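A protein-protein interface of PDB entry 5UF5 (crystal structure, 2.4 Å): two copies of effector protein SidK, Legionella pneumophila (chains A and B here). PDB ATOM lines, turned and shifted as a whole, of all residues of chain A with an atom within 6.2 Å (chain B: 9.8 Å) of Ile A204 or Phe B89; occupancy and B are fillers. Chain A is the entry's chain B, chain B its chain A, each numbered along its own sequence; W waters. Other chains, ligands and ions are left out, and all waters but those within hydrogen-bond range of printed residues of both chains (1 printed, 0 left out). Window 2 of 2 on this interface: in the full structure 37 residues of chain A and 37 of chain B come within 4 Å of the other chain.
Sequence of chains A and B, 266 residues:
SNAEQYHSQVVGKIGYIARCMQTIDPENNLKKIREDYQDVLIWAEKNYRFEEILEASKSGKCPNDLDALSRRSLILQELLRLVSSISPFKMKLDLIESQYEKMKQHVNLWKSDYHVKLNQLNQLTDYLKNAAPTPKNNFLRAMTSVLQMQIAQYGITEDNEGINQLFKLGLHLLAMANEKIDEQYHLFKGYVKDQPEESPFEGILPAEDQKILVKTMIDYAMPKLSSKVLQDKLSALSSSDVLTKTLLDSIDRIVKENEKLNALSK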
ATOM      1  N   ALA A 142     -36.536  -9.531  29.114  1.00  0.00           N
ATOM      2  CA  ALA A 142     -35.420  -9.289  30.022  1.00  0.00           C
ATOM      3  C   ALA A 142     -34.528 -10.519  30.134  1.00  0.00           C
ATOM      4  O   ALA A 142     -33.298 -10.402  30.103  1.00  0.00           O
ATOM      5  CB  ALA A 142     -35.938  -8.876  31.398  1.00  0.00           C
ATOM      6  N   THR A 144     -34.218 -12.940  27.918  1.00  0.00           N
ATOM      7  CA  THR A 144     -33.564 -13.195  26.638  1.00  0.00           C
ATOM      8  C   THR A 144     -32.386 -12.251  26.420  1.00  0.00           C
ATOM      9  O   THR A 144     -31.350 -12.658  25.880  1.00  0.00           O
ATOM     10  CB  THR A 144     -34.572 -13.072  25.494  1.00  0.00           C
ATOM     11  OG1 THR A 144     -35.669 -13.968  25.723  1.00  0.00           O
ATOM     12  CG2 THR A 144     -33.920 -13.417  24.161  1.00  0.00           C
ATOM     13  N   SER A 145     -32.521 -10.989  26.838  1.00  0.00           N
ATOM     14  CA  SER A 145     -31.421 -10.041  26.690  1.00  0.00           C
ATOM     15  C   SER A 145     -30.223 -10.451  27.537  1.00  0.00           C
ATOM     16  O   SER A 145     -29.073 -10.307  27.105  1.00  0.00           O
ATOM     17  CB  SER A 145     -31.883  -8.631  27.058  1.00  0.00           C
ATOM     18  OG  SER A 145     -32.811  -8.133  26.111  1.00  0.00           O
ATOM     19  N   VAL A 146     -30.471 -10.960  28.746  1.00  0.00           N
ATOM     20  CA  VAL A 146     -29.385 -11.501  29.558  1.00  0.00           C
ATOM     21  C   VAL A 146     -28.772 -12.713  28.870  1.00  0.00           C
ATOM     22  O   VAL A 146     -27.547 -12.891  28.861  1.00  0.00           O
ATOM     23  CB  VAL A 146     -29.891 -11.843  30.972  1.00  0.00           C
ATOM     24  CG1 VAL A 146     -28.765 -12.418  31.818  1.00  0.00           C
ATOM     25  CG2 VAL A 146     -30.485 -10.609  31.639  1.00  0.00           C
ATOM     26  N   LEU A 147     -29.615 -13.559  28.271  1.00  0.00           N
ATOM     27  CA  LEU A 147     -29.122 -14.725  27.544  1.00  0.00           C
ATOM     28  C   LEU A 147     -28.232 -14.315  26.378  1.00  0.00           C
ATOM     29  O   LEU A 147     -27.156 -14.891  26.174  1.00  0.00           O
ATOM     30  CB  LEU A 147     -30.303 -15.560  27.051  1.00  0.00           C
ATOM     31  CG  LEU A 147     -30.010 -16.769  26.162  1.00  0.00           C
ATOM     32  CD1 LEU A 147     -29.221 -17.822  26.918  1.00  0.00           C
ATOM     33  CD2 LEU A 147     -31.303 -17.353  25.636  1.00  0.00           C
ATOM     34  N   GLN A 148     -28.664 -13.316  25.602  1.00  0.00           N
ATOM     35  CA  GLN A 148     -27.873 -12.849  24.469  1.00  0.00           C
ATOM     36  C   GLN A 148     -26.542 -12.267  24.925  1.00  0.00           C
ATOM     37  O   GLN A 148     -25.510 -12.469  24.272  1.00  0.00           O
ATOM     38  CB  GLN A 148     -28.661 -11.808  23.676  1.00  0.00           C
ATOM     39  CG  GLN A 148     -29.803 -12.380  22.861  1.00  0.00           C
ATOM     40  CD  GLN A 148     -30.606 -11.302  22.164  1.00  0.00           C
ATOM     41  OE1 GLN A 148     -30.981 -10.302  22.776  1.00  0.00           O
ATOM     42  NE2 GLN A 148     -30.866 -11.493  20.876  1.00  0.00           N
ATOM     43  N   MET A 149     -26.545 -11.535  26.041  1.00  0.00           N
ATOM     44  CA  MET A 149     -25.305 -10.964  26.551  1.00  0.00           C
ATOM     45  C   MET A 149     -24.341 -12.054  27.000  1.00  0.00           C
ATOM     46  O   MET A 149     -23.130 -11.956  26.766  1.00  0.00           O
ATOM     47  CB  MET A 149     -25.610  -9.994  27.695  1.00  0.00           C
ATOM     48  CG  MET A 149     -24.387  -9.412  28.395  1.00  0.00           C
ATOM     49  SD  MET A 149     -23.839 -10.409  29.797  1.00  0.00           S
ATOM     50  CE  MET A 149     -22.492  -9.411  30.432  1.00  0.00           C
ATOM     51  N   ALA A 152     -22.837 -13.857  24.045  1.00  0.00           N
ATOM     52  CA  ALA A 152     -21.806 -13.003  23.471  1.00  0.00           C
ATOM     53  C   ALA A 152     -20.485 -13.147  24.214  1.00  0.00           C
ATOM     54  O   ALA A 152     -19.414 -13.015  23.611  1.00  0.00           O
ATOM     55  CB  ALA A 152     -22.267 -11.546  23.483  1.00  0.00           C
ATOM     56  N   PRO A 200     -28.960  -8.295  37.733  1.00  0.00           N
ATOM     57  CA  PRO A 200     -28.609  -9.001  36.487  1.00  0.00           C
ATOM     58  C   PRO A 200     -28.941  -8.241  35.216  1.00  0.00           C
ATOM     59  O   PRO A 200     -28.439  -8.620  34.150  1.00  0.00           O
ATOM     60  CB  PRO A 200     -29.426 -10.298  36.580  1.00  0.00           C
ATOM     61  CG  PRO A 200     -30.570  -9.961  37.478  1.00  0.00           C
ATOM     62  CD  PRO A 200     -30.063  -8.944  38.458  1.00  0.00           C
ATOM     63  N   PHE A 201     -29.758  -7.196  35.289  1.00  0.00           N
ATOM     64  CA  PHE A 201     -30.204  -6.465  34.111  1.00  0.00           C
ATOM     65  C   PHE A 201     -29.460  -5.155  33.899  1.00  0.00           C
ATOM     66  O   PHE A 201     -29.767  -4.435  32.943  1.00  0.00           O
ATOM     67  CB  PHE A 201     -31.710  -6.191  34.200  1.00  0.00           C
ATOM     68  CG  PHE A 201     -32.526  -7.406  34.541  1.00  0.00           C
ATOM     69  CD1 PHE A 201     -32.528  -8.510  33.702  1.00  0.00           C
ATOM     70  CD2 PHE A 201     -33.301  -7.442  35.689  1.00  0.00           C
ATOM     71  CE1 PHE A 201     -33.279  -9.630  34.009  1.00  0.00           C
ATOM     72  CE2 PHE A 201     -34.059  -8.560  35.999  1.00  0.00           C
ATOM     73  CZ  PHE A 201     -34.047  -9.656  35.157  1.00  0.00           C
ATOM     74  N   GLU A 202     -28.498  -4.827  34.759  1.00  0.00           N
ATOM     75  CA  GLU A 202     -27.748  -3.586  34.614  1.00  0.00           C
ATOM     76  C   GLU A 202     -26.867  -3.643  33.373  1.00  0.00           C
ATOM     77  O   GLU A 202     -26.185  -4.644  33.129  1.00  0.00           O
ATOM     78  CB  GLU A 202     -26.896  -3.329  35.856  1.00  0.00           C
ATOM     79  N   GLY A 203     -26.888  -2.569  32.586  1.00  0.00           N
ATOM     80  CA  GLY A 203     -26.130  -2.505  31.354  1.00  0.00           C
ATOM     81  C   GLY A 203     -26.602  -3.425  30.251  1.00  0.00           C
ATOM     82  O   GLY A 203     -25.999  -3.428  29.172  1.00  0.00           O
ATOM     83  N   ILE A 204     -27.660  -4.201  30.481  1.00  0.00           N
ATOM     84  CA  ILE A 204     -28.156  -5.144  29.495  1.00  0.00           C
ATOM     85  C   ILE A 204     -29.481  -4.703  28.880  1.00  0.00           C
ATOM     86  O   ILE A 204     -29.705  -4.939  27.687  1.00  0.00           O
ATOM     87  CB  ILE A 204     -28.280  -6.547  30.122  1.00  0.00           C
ATOM     88  CG1 ILE A 204     -26.915  -7.011  30.637  1.00  0.00           C
ATOM     89  CG2 ILE A 204     -28.847  -7.548  29.126  1.00  0.00           C
ATOM     90  CD1 ILE A 204     -26.923  -8.398  31.240  1.00  0.00           C
ATOM     91  N   LEU A 205     -30.355  -4.060  29.649  1.00  0.00           N
ATOM     92  CA  LEU A 205     -31.616  -3.546  29.147  1.00  0.00           C
ATOM     93  C   LEU A 205     -31.650  -2.026  29.272  1.00  0.00           C
ATOM     94  O   LEU A 205     -30.988  -1.457  30.147  1.00  0.00           O
ATOM     95  CB  LEU A 205     -32.803  -4.151  29.909  1.00  0.00           C
ATOM     96  N   PRO A 206     -32.395  -1.342  28.401  1.00  0.00           N
ATOM     97  CA  PRO A 206     -32.523   0.114  28.529  1.00  0.00           C
ATOM     98  C   PRO A 206     -33.100   0.505  29.881  1.00  0.00           C
ATOM     99  O   PRO A 206     -33.812  -0.268  30.526  1.00  0.00           O
ATOM    100  CB  PRO A 206     -33.473   0.487  27.386  1.00  0.00           C
ATOM    101  CG  PRO A 206     -33.307  -0.609  26.389  1.00  0.00           C
ATOM    102  CD  PRO A 206     -33.057  -1.854  27.189  1.00  0.00           C
ATOM    103  N   GLN A 210     -36.010  -1.203  32.519  1.00  0.00           N
ATOM    104  CA  GLN A 210     -35.725  -1.638  33.882  1.00  0.00           C
ATOM    105  C   GLN A 210     -36.731  -1.073  34.876  1.00  0.00           C
ATOM    106  O   GLN A 210     -37.051  -1.732  35.872  1.00  0.00           O
ATOM    107  CB  GLN A 210     -34.306  -1.237  34.281  1.00  0.00           C
ATOM    108  CG  GLN A 210     -33.224  -1.804  33.383  1.00  0.00           C
ATOM    109  CD  GLN A 210     -31.903  -1.964  34.107  1.00  0.00           C
ATOM    110  OE1 GLN A 210     -31.853  -2.505  35.212  1.00  0.00           O
ATOM    111  NE2 GLN A 210     -30.827  -1.490  33.490  1.00  0.00           N
ATOM    112  N   LEU B  80     -23.195 -17.002  10.945  1.00  0.00           N
ATOM    113  CA  LEU B  80     -23.930 -15.749  10.801  1.00  0.00           C
ATOM    114  C   LEU B  80     -25.166 -15.729  11.693  1.00  0.00           C
ATOM    115  O   LEU B  80     -25.489 -14.694  12.287  1.00  0.00           O
ATOM    116  CB  LEU B  80     -24.320 -15.526   9.341  1.00  0.00           C
ATOM    117  CG  LEU B  80     -25.150 -14.273   9.050  1.00  0.00           C
ATOM    118  CD1 LEU B  80     -24.461 -13.023   9.575  1.00  0.00           C
ATOM    119  CD2 LEU B  80     -25.431 -14.144   7.559  1.00  0.00           C
ATOM    120  N   ARG B  81     -25.865 -16.865  11.802  1.00  0.00           N
ATOM    121  CA  ARG B  81     -27.040 -16.939  12.670  1.00  0.00           C
ATOM    122  C   ARG B  81     -26.691 -16.576  14.107  1.00  0.00           C
ATOM    123  O   ARG B  81     -27.434 -15.839  14.763  1.00  0.00           O
ATOM    124  CB  ARG B  81     -27.654 -18.338  12.625  1.00  0.00           C
ATOM    125  CG  ARG B  81     -28.692 -18.558  11.548  1.00  0.00           C
ATOM    126  CD  ARG B  81     -29.225 -19.981  11.619  1.00  0.00           C
ATOM    127  NE  ARG B  81     -30.085 -20.192  12.779  1.00  0.00           N
ATOM    128  CZ  ARG B  81     -30.226 -21.360  13.401  1.00  0.00           C
ATOM    129  NH1 ARG B  81     -29.549 -22.420  12.987  1.00  0.00           N
ATOM    130  NH2 ARG B  81     -31.037 -21.463  14.445  1.00  0.00           N
ATOM    131  N   LEU B  82     -25.572 -17.096  14.616  1.00  0.00           N
ATOM    132  CA  LEU B  82     -25.173 -16.804  15.990  1.00  0.00           C
ATOM    133  C   LEU B  82     -24.901 -15.319  16.178  1.00  0.00           C
ATOM    134  O   LEU B  82     -25.451 -14.681  17.085  1.00  0.00           O
ATOM    135  CB  LEU B  82     -23.939 -17.628  16.360  1.00  0.00           C
ATOM    136  CG  LEU B  82     -23.260 -17.266  17.681  1.00  0.00           C
ATOM    137  CD1 LEU B  82     -24.229 -17.421  18.845  1.00  0.00           C
ATOM    138  CD2 LEU B  82     -22.017 -18.116  17.898  1.00  0.00           C
ATOM    139  N   VAL B  83     -24.050 -14.751  15.322  1.00  0.00           N
ATOM    140  CA  VAL B  83     -23.699 -13.338  15.421  1.00  0.00           C
ATOM    141  C   VAL B  83     -24.939 -12.464  15.283  1.00  0.00           C
ATOM    142  O   VAL B  83     -25.084 -11.447  15.974  1.00  0.00           O
ATOM    143  CB  VAL B  83     -22.633 -12.998  14.362  1.00  0.00           C
ATOM    144  CG1 VAL B  83     -22.620 -11.510  14.063  1.00  0.00           C
ATOM    145  CG2 VAL B  83     -21.265 -13.478  14.830  1.00  0.00           C
ATOM    146  N   SER B  84     -25.864 -12.860  14.409  1.00  0.00           N
ATOM    147  CA  SER B  84     -27.056 -12.058  14.164  1.00  0.00           C
ATOM    148  C   SER B  84     -28.102 -12.215  15.263  1.00  0.00           C
ATOM    149  O   SER B  84     -28.854 -11.272  15.529  1.00  0.00           O
ATOM    150  CB  SER B  84     -27.657 -12.428  12.808  1.00  0.00           C
ATOM    151  OG  SER B  84     -28.895 -11.778  12.605  1.00  0.00           O
ATOM    152  N   SER B  85     -28.160 -13.378  15.917  1.00  0.00           N
ATOM    153  CA  SER B  85     -29.208 -13.658  16.893  1.00  0.00           C
ATOM    154  C   SER B  85     -28.923 -13.086  18.277  1.00  0.00           C
ATOM    155  O   SER B  85     -29.843 -13.031  19.102  1.00  0.00           O
ATOM    156  CB  SER B  85     -29.430 -15.167  17.009  1.00  0.00           C
ATOM    157  OG  SER B  85     -29.846 -15.715  15.768  1.00  0.00           O
ATOM    158  N   ILE B  86     -27.686 -12.673  18.560  1.00  0.00           N
ATOM    159  CA  ILE B  86     -27.365 -12.071  19.852  1.00  0.00           C
ATOM    160  C   ILE B  86     -27.311 -10.552  19.794  1.00  0.00           C
ATOM    161  O   ILE B  86     -27.132  -9.914  20.844  1.00  0.00           O
ATOM    162  CB  ILE B  86     -26.031 -12.609  20.409  1.00  0.00           C
ATOM    163  CG1 ILE B  86     -24.901 -12.366  19.407  1.00  0.00           C
ATOM    164  CG2 ILE B  86     -26.158 -14.086  20.764  1.00  0.00           C
ATOM    165  CD1 ILE B  86     -23.527 -12.511  19.994  1.00  0.00           C
ATOM    166  N   SER B  87     -27.446  -9.955  18.612  1.00  0.00           N
ATOM    167  CA  SER B  87     -27.485  -8.503  18.456  1.00  0.00           C
ATOM    168  C   SER B  87     -28.532  -7.897  19.389  1.00  0.00           C
ATOM    169  O   SER B  87     -29.599  -8.482  19.576  1.00  0.00           O
ATOM    170  CB  SER B  87     -27.782  -8.144  16.996  1.00  0.00           C
ATOM    171  OG  SER B  87     -27.899  -6.744  16.811  1.00  0.00           O
ATOM    172  N   PRO B  88     -28.246  -6.716  19.970  1.00  0.00           N
ATOM    173  CA  PRO B  88     -27.120  -5.806  19.719  1.00  0.00           C
ATOM    174  C   PRO B  88     -25.800  -6.181  20.397  1.00  0.00           C
ATOM    175  O   PRO B  88     -24.790  -5.523  20.148  1.00  0.00           O
ATOM    176  CB  PRO B  88     -27.632  -4.479  20.277  1.00  0.00           C
ATOM    177  CG  PRO B  88     -28.492  -4.892  21.420  1.00  0.00           C
ATOM    178  CD  PRO B  88     -29.150  -6.182  21.006  1.00  0.00           C
ATOM    179  N   PHE B  89     -25.806  -7.207  21.243  1.00  0.00           N
ATOM    180  CA  PHE B  89     -24.577  -7.632  21.897  1.00  0.00           C
ATOM    181  C   PHE B  89     -23.625  -8.245  20.876  1.00  0.00           C
ATOM    182  O   PHE B  89     -24.050  -8.900  19.922  1.00  0.00           O
ATOM    183  CB  PHE B  89     -24.889  -8.634  23.007  1.00  0.00           C
ATOM    184  CG  PHE B  89     -25.911  -8.140  23.989  1.00  0.00           C
ATOM    185  CD1 PHE B  89     -25.534  -7.347  25.060  1.00  0.00           C
ATOM    186  CD2 PHE B  89     -27.250  -8.456  23.834  1.00  0.00           C
ATOM    187  CE1 PHE B  89     -26.476  -6.886  25.963  1.00  0.00           C
ATOM    188  CE2 PHE B  89     -28.193  -7.998  24.732  1.00  0.00           C
ATOM    189  CZ  PHE B  89     -27.806  -7.211  25.797  1.00  0.00           C
ATOM    190  N   LYS B  90     -22.330  -8.022  21.075  1.00  0.00           N
ATOM    191  CA  LYS B  90     -21.326  -8.473  20.127  1.00  0.00           C
ATOM    192  C   LYS B  90     -20.343  -9.427  20.792  1.00  0.00           C
ATOM    193  O   LYS B  90     -20.214  -9.476  22.019  1.00  0.00           O
ATOM    194  CB  LYS B  90     -20.575  -7.291  19.499  1.00  0.00           C
ATOM    195  CG  LYS B  90     -21.149  -6.857  18.158  1.00  0.00           C
ATOM    196  CD  LYS B  90     -21.661  -5.429  18.199  1.00  0.00           C
ATOM    197  CE  LYS B  90     -22.486  -5.104  16.963  1.00  0.00           C
ATOM    198  NZ  LYS B  90     -21.783  -5.479  15.703  1.00  0.00           N
ATOM    199  N   MET B  91     -19.643 -10.178  19.950  1.00  0.00           N
ATOM    200  CA  MET B  91     -18.776 -11.268  20.364  1.00  0.00           C
ATOM    201  C   MET B  91     -17.327 -10.929  20.037  1.00  0.00           C
ATOM    202  O   MET B  91     -17.040 -10.347  18.987  1.00  0.00           O
ATOM    203  CB  MET B  91     -19.200 -12.556  19.657  1.00  0.00           C
ATOM    204  CG  MET B  91     -18.524 -13.817  20.121  1.00  0.00           C
ATOM    205  SD  MET B  91     -19.340 -15.253  19.396  1.00  0.00           S
ATOM    206  CE  MET B  91     -20.975 -15.098  20.105  1.00  0.00           C
ATOM    207  N   LYS B  92     -16.418 -11.286  20.944  1.00  0.00           N
ATOM    208  CA  LYS B  92     -14.999 -11.079  20.687  1.00  0.00           C
ATOM    209  C   LYS B  92     -14.539 -11.943  19.519  1.00  0.00           C
ATOM    210  O   LYS B  92     -15.040 -13.050  19.299  1.00  0.00           O
ATOM    211  CB  LYS B  92     -14.169 -11.390  21.932  1.00  0.00           C
ATOM    212  CG  LYS B  92     -14.319 -10.365  23.042  1.00  0.00           C
ATOM    213  CD  LYS B  92     -13.002 -10.128  23.756  1.00  0.00           C
ATOM    214  CE  LYS B  92     -13.031 -10.657  25.176  1.00  0.00           C
ATOM    215  NZ  LYS B  92     -11.884 -10.129  25.973  1.00  0.00           N
ATOM    216  N   ILE B  96     -15.471 -15.766  18.209  1.00  0.00           N
ATOM    217  CA  ILE B  96     -16.137 -16.044  16.937  1.00  0.00           C
ATOM    218  C   ILE B  96     -15.408 -17.155  16.188  1.00  0.00           C
ATOM    219  O   ILE B  96     -16.026 -18.111  15.706  1.00  0.00           O
ATOM    220  CB  ILE B  96     -16.233 -14.766  16.086  1.00  0.00           C
ATOM    221  CG1 ILE B  96     -17.048 -13.696  16.812  1.00  0.00           C
ATOM    222  CG2 ILE B  96     -16.851 -15.079  14.735  1.00  0.00           C
ATOM    223  CD1 ILE B  96     -17.131 -12.386  16.058  1.00  0.00           C
HETATM  224  O   HOH W   1     -16.769 -12.318  23.707  1.00  0.00           O
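Ser A145 touches Phe B89.
Gln A148 touches Ile B86.
Gln A148 touches Ser B87.
CB of Gln A148 touches CD2 of Phe B89, at 3.6 Å.
Phe B89 touches Met A149 (CE1 to CB, 3.7 Å).
CB of Ala A152 touches CD1 of Ile B86 (3.8 Å).
Ala A152 touches Phe B89.
Lys B90 touches Ala A152.
CG of Met B91 touches O of Ala A152, 3.7 Å away.
CZ of Phe B89 touches CG2 of Ile A204 (3.5 Å).
The backbone carbonyl oxygen (O) of Arg B81 sits at hydrogen-bond distance from the side-chain hydroxyl (OG) of Ser B85, 2.6 Å away.
Printed residues of chain B within 4 Å of Ile A204: Phe B89.
Phe B89 touches just these residues of chain A: Ser A145, Gln A148, Met A149, Ala A152 and Ile A204.
Ser A145 touches just one residue of chain B: Phe B89 (3.4 Å).
No residue of chain B comes within 4 Å of Val A146.
Printed residues of chain B within 4 Å of Gln A148: Ser B85 (2.6 Å), Ile B86 (3.7 Å), Ser B87 (3.5 Å) and Phe B89 (3.6 Å).
Met A149 touches just one residue of chain B: Phe B89.
No residue of chain B comes within 4 Å of Glu A202.
No residue of chain B comes within 4 Å of Gly A203.
Leu A205 touches none of the printed residues of chain B.
Printed residues of chain B within 4 Å of Ala A152: Ile B86 (3.8 Å), Phe B89 (3.9 Å), Lys B90 (3.3 Å) and Met B91 (3.7 Å).
Of the printed residues of chain A, Ser B87 touches Gln A148 (3.5 Å).
Of the printed residues of chain A, Ile B86 touches Gln A148 (3.7 Å) and Ala A152 (3.8 Å).
Of the printed residues of chain A, Lys B90 touches Ala A152.
Water W1 lies within hydrogen-bond range of O of Ala A152 (2.7 Å) and N of Lys B92 (3.0 Å).
No position is printed for both chains.
The backbone carbonyl oxygen (O) of Ser B85 lies within hydrogen-bond range of the side-chain amide nitrogen (NE2) of Gln A148.
Along chain A the printed residues that touch a printed residue of chain B span positions 145 to 204.
Of the 14 printed residues of chain B, 6 touch a printed residue of chain A.
Hydrophobic or aromatic side chains of chain B that line the printed part of chain A: Ile B86, Phe B89 and Met B91.
Among the printed residues, 11 pairs touch across the chains.
Among the printed residues, no Asp or Glu carboxylate lies within 4 Å of a Lys or Arg side-chain nitrogen of the other chain.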
